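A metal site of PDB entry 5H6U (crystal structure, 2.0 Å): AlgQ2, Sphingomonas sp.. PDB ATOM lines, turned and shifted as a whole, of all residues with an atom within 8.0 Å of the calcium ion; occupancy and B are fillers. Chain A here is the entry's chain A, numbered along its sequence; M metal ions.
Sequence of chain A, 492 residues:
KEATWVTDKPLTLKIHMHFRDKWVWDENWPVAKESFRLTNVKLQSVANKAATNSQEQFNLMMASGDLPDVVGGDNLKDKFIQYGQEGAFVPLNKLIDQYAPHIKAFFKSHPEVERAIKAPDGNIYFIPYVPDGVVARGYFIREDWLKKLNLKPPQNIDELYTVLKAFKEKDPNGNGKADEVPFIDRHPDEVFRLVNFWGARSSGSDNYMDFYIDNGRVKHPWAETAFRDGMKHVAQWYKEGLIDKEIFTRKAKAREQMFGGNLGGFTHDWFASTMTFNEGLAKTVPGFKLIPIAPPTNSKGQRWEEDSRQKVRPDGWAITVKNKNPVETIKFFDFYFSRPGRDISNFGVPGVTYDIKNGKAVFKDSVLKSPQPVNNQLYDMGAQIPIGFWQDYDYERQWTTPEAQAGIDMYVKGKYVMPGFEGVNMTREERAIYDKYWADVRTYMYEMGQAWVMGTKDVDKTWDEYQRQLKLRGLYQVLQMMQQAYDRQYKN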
ATOM      1  N   TRP A 145       5.619  29.156 -16.930  1.00  0.00           N
ATOM      2  CA  TRP A 145       6.562  28.167 -16.412  1.00  0.00           C
ATOM      3  C   TRP A 145       7.702  27.934 -17.409  1.00  0.00           C
ATOM      4  O   TRP A 145       8.854  27.803 -17.007  1.00  0.00           O
ATOM      5  CB  TRP A 145       5.856  26.853 -16.088  1.00  0.00           C
ATOM      6  CG  TRP A 145       5.046  26.925 -14.872  1.00  0.00           C
ATOM      7  CD1 TRP A 145       4.807  28.033 -14.112  1.00  0.00           C
ATOM      8  CD2 TRP A 145       4.317  25.853 -14.259  1.00  0.00           C
ATOM      9  NE1 TRP A 145       3.990  27.710 -13.053  1.00  0.00           N
ATOM     10  CE2 TRP A 145       3.690  26.377 -13.119  1.00  0.00           C
ATOM     11  CE3 TRP A 145       4.176  24.485 -14.558  1.00  0.00           C
ATOM     12  CZ2 TRP A 145       2.895  25.593 -12.281  1.00  0.00           C
ATOM     13  CZ3 TRP A 145       3.377  23.700 -13.707  1.00  0.00           C
ATOM     14  CH2 TRP A 145       2.750  24.256 -12.586  1.00  0.00           C
ATOM     15  N   PHE A 167       8.631  20.495 -15.601  1.00  0.00           N
ATOM     16  CA  PHE A 167       7.560  21.002 -14.732  1.00  0.00           C
ATOM     17  C   PHE A 167       7.521  20.210 -13.450  1.00  0.00           C
ATOM     18  O   PHE A 167       7.391  20.782 -12.349  1.00  0.00           O
ATOM     19  CB  PHE A 167       6.207  20.920 -15.427  1.00  0.00           C
ATOM     20  CG  PHE A 167       6.001  21.930 -16.497  1.00  0.00           C
ATOM     21  CD1 PHE A 167       6.924  22.932 -16.697  1.00  0.00           C
ATOM     22  CD2 PHE A 167       4.899  21.855 -17.341  1.00  0.00           C
ATOM     23  CE1 PHE A 167       6.747  23.874 -17.687  1.00  0.00           C
ATOM     24  CE2 PHE A 167       4.697  22.789 -18.364  1.00  0.00           C
ATOM     25  CZ  PHE A 167       5.622  23.799 -18.533  1.00  0.00           C
ATOM     26  N   LYS A 168       7.666  18.888 -13.579  1.00  0.00           N
ATOM     27  CA  LYS A 168       7.578  17.989 -12.439  1.00  0.00           C
ATOM     28  C   LYS A 168       8.725  18.214 -11.479  1.00  0.00           C
ATOM     29  O   LYS A 168       8.514  18.352 -10.271  1.00  0.00           O
ATOM     30  CB  LYS A 168       7.574  16.550 -12.930  1.00  0.00           C
ATOM     31  CG  LYS A 168       7.336  15.525 -11.844  1.00  0.00           C
ATOM     32  CD  LYS A 168       5.886  15.537 -11.377  1.00  0.00           C
ATOM     33  CE  LYS A 168       5.626  14.412 -10.400  1.00  0.00           C
ATOM     34  NZ  LYS A 168       6.487  14.596  -9.156  1.00  0.00           N
ATOM     35  N   GLU A 169       9.962  18.245 -11.998  1.00  0.00           N
ATOM     36  CA  GLU A 169      11.160  18.094 -11.186  1.00  0.00           C
ATOM     37  C   GLU A 169      11.821  19.394 -10.771  1.00  0.00           C
ATOM     38  O   GLU A 169      12.626  19.388  -9.840  1.00  0.00           O
ATOM     39  CB  GLU A 169      12.189  17.253 -11.947  1.00  0.00           C
ATOM     40  CG  GLU A 169      11.715  15.858 -12.303  1.00  0.00           C
ATOM     41  CD  GLU A 169      12.791  15.062 -13.003  1.00  0.00           C
ATOM     42  OE1 GLU A 169      12.763  13.823 -12.876  1.00  0.00           O
ATOM     43  OE2 GLU A 169      13.667  15.668 -13.663  1.00  0.00           O
ATOM     44  N   LYS A 170      11.517  20.502 -11.420  1.00  0.00           N
ATOM     45  CA  LYS A 170      12.286  21.719 -11.163  1.00  0.00           C
ATOM     46  C   LYS A 170      11.420  22.879 -10.681  1.00  0.00           C
ATOM     47  O   LYS A 170      11.684  24.031 -11.025  1.00  0.00           O
ATOM     48  CB  LYS A 170      13.086  22.120 -12.395  1.00  0.00           C
ATOM     49  CG  LYS A 170      14.371  21.304 -12.574  1.00  0.00           C
ATOM     50  CD  LYS A 170      15.574  22.207 -12.871  1.00  0.00           C
ATOM     51  CE  LYS A 170      15.972  23.043 -11.647  1.00  0.00           C
ATOM     52  NZ  LYS A 170      16.524  22.231 -10.520  1.00  0.00           N
ATOM     53  N   ASP A 171      10.392  22.580  -9.887  1.00  0.00           N
ATOM     54  CA  ASP A 171       9.695  23.567  -9.057  1.00  0.00           C
ATOM     55  C   ASP A 171       9.342  24.889  -9.740  1.00  0.00           C
ATOM     56  O   ASP A 171       9.651  25.963  -9.205  1.00  0.00           O
ATOM     57  CB  ASP A 171      10.548  23.823  -7.824  1.00  0.00           C
ATOM     58  CG  ASP A 171       9.823  24.625  -6.766  1.00  0.00           C
ATOM     59  OD1 ASP A 171       8.620  24.376  -6.584  1.00  0.00           O
ATOM     60  OD2 ASP A 171      10.444  25.514  -6.151  1.00  0.00           O
ATOM     61  N   PRO A 172       8.678  24.858 -10.895  1.00  0.00           N
ATOM     62  CA  PRO A 172       8.356  26.139 -11.563  1.00  0.00           C
ATOM     63  C   PRO A 172       7.460  27.067 -10.768  1.00  0.00           C
ATOM     64  O   PRO A 172       7.501  28.278 -11.014  1.00  0.00           O
ATOM     65  CB  PRO A 172       7.695  25.692 -12.882  1.00  0.00           C
ATOM     66  CG  PRO A 172       7.307  24.261 -12.672  1.00  0.00           C
ATOM     67  CD  PRO A 172       8.329  23.704 -11.741  1.00  0.00           C
ATOM     68  N   ASN A 173       6.638  26.565  -9.835  1.00  0.00           N
ATOM     69  CA  ASN A 173       5.889  27.526  -9.050  1.00  0.00           C
ATOM     70  C   ASN A 173       6.703  28.132  -7.909  1.00  0.00           C
ATOM     71  O   ASN A 173       6.199  29.056  -7.242  1.00  0.00           O
ATOM     72  CB  ASN A 173       4.574  26.938  -8.505  1.00  0.00           C
ATOM     73  CG  ASN A 173       4.749  25.758  -7.548  1.00  0.00           C
ATOM     74  OD1 ASN A 173       5.797  25.546  -6.949  1.00  0.00           O
ATOM     75  ND2 ASN A 173       3.670  24.970  -7.397  1.00  0.00           N
ATOM     76  N   GLY A 174       7.920  27.657  -7.692  1.00  0.00           N
ATOM     77  CA  GLY A 174       8.841  28.241  -6.725  1.00  0.00           C
ATOM     78  C   GLY A 174       8.280  28.278  -5.330  1.00  0.00           C
ATOM     79  O   GLY A 174       8.030  29.346  -4.767  1.00  0.00           O
ATOM     80  N   ASN A 175       8.033  27.104  -4.763  1.00  0.00           N
ATOM     81  CA  ASN A 175       7.656  26.972  -3.370  1.00  0.00           C
ATOM     82  C   ASN A 175       8.457  25.868  -2.720  1.00  0.00           C
ATOM     83  O   ASN A 175       8.083  25.376  -1.652  1.00  0.00           O
ATOM     84  CB  ASN A 175       6.150  26.734  -3.223  1.00  0.00           C
ATOM     85  CG  ASN A 175       5.663  25.466  -3.949  1.00  0.00           C
ATOM     86  OD1 ASN A 175       6.445  24.587  -4.342  1.00  0.00           O
ATOM     87  ND2 ASN A 175       4.352  25.347  -4.080  1.00  0.00           N
ATOM     88  N   GLY A 176       9.539  25.439  -3.366  1.00  0.00           N
ATOM     89  CA  GLY A 176      10.383  24.389  -2.853  1.00  0.00           C
ATOM     90  C   GLY A 176       9.805  23.001  -2.883  1.00  0.00           C
ATOM     91  O   GLY A 176      10.541  22.038  -2.643  1.00  0.00           O
ATOM     92  N   LYS A 177       8.513  22.850  -3.192  1.00  0.00           N
ATOM     93  CA  LYS A 177       7.833  21.561  -3.121  1.00  0.00           C
ATOM     94  C   LYS A 177       7.636  20.954  -4.505  1.00  0.00           C
ATOM     95  O   LYS A 177       7.411  21.673  -5.483  1.00  0.00           O
ATOM     96  CB  LYS A 177       6.479  21.682  -2.434  1.00  0.00           C
ATOM     97  CG  LYS A 177       6.512  22.426  -1.126  1.00  0.00           C
ATOM     98  CD  LYS A 177       5.179  22.300  -0.373  1.00  0.00           C
ATOM     99  CE  LYS A 177       3.971  22.471  -1.277  1.00  0.00           C
ATOM    100  NZ  LYS A 177       2.695  22.332  -0.496  1.00  0.00           N
ATOM    101  N   ALA A 178       7.698  19.625  -4.574  1.00  0.00           N
ATOM    102  CA  ALA A 178       7.399  18.922  -5.809  1.00  0.00           C
ATOM    103  C   ALA A 178       5.902  18.651  -5.834  1.00  0.00           C
ATOM    104  O   ALA A 178       5.412  17.530  -5.714  1.00  0.00           O
ATOM    105  CB  ALA A 178       8.224  17.645  -5.939  1.00  0.00           C
ATOM    106  N   ASP A 179       5.171  19.745  -5.975  1.00  0.00           N
ATOM    107  CA  ASP A 179       3.724  19.679  -6.038  1.00  0.00           C
ATOM    108  C   ASP A 179       3.197  19.806  -7.452  1.00  0.00           C
ATOM    109  O   ASP A 179       1.991  19.655  -7.647  1.00  0.00           O
ATOM    110  CB  ASP A 179       3.101  20.772  -5.155  1.00  0.00           C
ATOM    111  CG  ASP A 179       3.579  22.158  -5.510  1.00  0.00           C
ATOM    112  OD1 ASP A 179       4.662  22.279  -6.136  1.00  0.00           O
ATOM    113  OD2 ASP A 179       2.883  23.130  -5.136  1.00  0.00           O
ATOM    114  N   GLU A 180       4.062  20.103  -8.436  1.00  0.00           N
ATOM    115  CA  GLU A 180       3.618  20.346  -9.801  1.00  0.00           C
ATOM    116  C   GLU A 180       3.061  19.076 -10.416  1.00  0.00           C
ATOM    117  O   GLU A 180       3.663  17.996 -10.314  1.00  0.00           O
ATOM    118  CB  GLU A 180       4.760  20.856 -10.683  1.00  0.00           C
ATOM    119  CG  GLU A 180       5.026  22.332 -10.554  1.00  0.00           C
ATOM    120  CD  GLU A 180       5.824  22.686  -9.308  1.00  0.00           C
ATOM    121  OE1 GLU A 180       6.172  23.875  -9.201  1.00  0.00           O
ATOM    122  OE2 GLU A 180       6.084  21.798  -8.441  1.00  0.00           O
ATOM    123  N   VAL A 181       1.968  19.221 -11.144  1.00  0.00           N
ATOM    124  CA  VAL A 181       1.319  18.130 -11.844  1.00  0.00           C
ATOM    125  C   VAL A 181       1.276  18.469 -13.331  1.00  0.00           C
ATOM    126  O   VAL A 181       0.418  19.212 -13.789  1.00  0.00           O
ATOM    127  CB  VAL A 181      -0.084  17.881 -11.280  1.00  0.00           C
ATOM    128  CG1 VAL A 181      -0.793  16.778 -12.063  1.00  0.00           C
ATOM    129  CG2 VAL A 181       0.044  17.563  -9.797  1.00  0.00           C
ATOM    130  N   ASN A 262      -2.247  26.561  -9.115  1.00  0.00           N
ATOM    131  CA  ASN A 262      -0.902  26.699  -9.673  1.00  0.00           C
ATOM    132  C   ASN A 262      -0.119  25.380  -9.589  1.00  0.00           C
ATOM    133  O   ASN A 262       1.081  25.362  -9.309  1.00  0.00           O
ATOM    134  CB  ASN A 262      -0.145  27.831  -8.976  1.00  0.00           C
ATOM    135  CG  ASN A 262       1.035  28.365  -9.796  1.00  0.00           C
ATOM    136  OD1 ASN A 262       1.131  28.167 -11.022  1.00  0.00           O
ATOM    137  ND2 ASN A 262       1.933  29.047  -9.108  1.00  0.00           N
ATOM    138  N   LEU A 263      -0.807  24.279  -9.895  1.00  0.00           N
ATOM    139  CA  LEU A 263      -0.174  22.968  -9.896  1.00  0.00           C
ATOM    140  C   LEU A 263      -0.022  22.365 -11.287  1.00  0.00           C
ATOM    141  O   LEU A 263       0.884  21.549 -11.500  1.00  0.00           O
ATOM    142  CB  LEU A 263      -0.982  21.991  -9.037  1.00  0.00           C
ATOM    143  CG  LEU A 263      -1.233  22.428  -7.593  1.00  0.00           C
ATOM    144  CD1 LEU A 263      -2.094  21.355  -6.885  1.00  0.00           C
ATOM    145  CD2 LEU A 263       0.102  22.623  -6.923  1.00  0.00           C
HETATM  146 CA    CA M   1       6.553  23.477  -6.604  1.00  0.00          CA
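Within 4 Å of the calcium ion: Asp 171, Asn 173, Asn 175, Lys 177, Asp 179 and Glu 180.
Along chain A the residues within 4 Å of the calcium ion span positions 171 to 180.
The backbone NH (N) of Gly 176 is in hydrogen-bond range of the side-chain carboxylate (OD2) of Asp 171 (2.9 Å).
The side-chain amide nitrogen of Asn 173 is in hydrogen-bond range of the backbone carbonyl oxygen of Asn 262 (3.2 Å).
The calcium ion is bound by the side-chain amide oxygen (OD1) of Asn 173 (2.2 Å), the side-chain carboxylate (OD1) of Asp 171 (2.3 Å), the side-chain carboxylate (OD1) of Asp 179 (2.3 Å), the backbone carbonyl oxygen (O) of Lys 177 (2.3 Å), the side-chain amide oxygen (OD1) of Asn 175 (2.5 Å), the side-chain carboxylate (OE2) of Glu 180 (2.5 Å) and the side-chain carboxylate (OE1) of Glu 180 (2.7 Å).
The calcium ion has seven donor atoms within binding distance.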
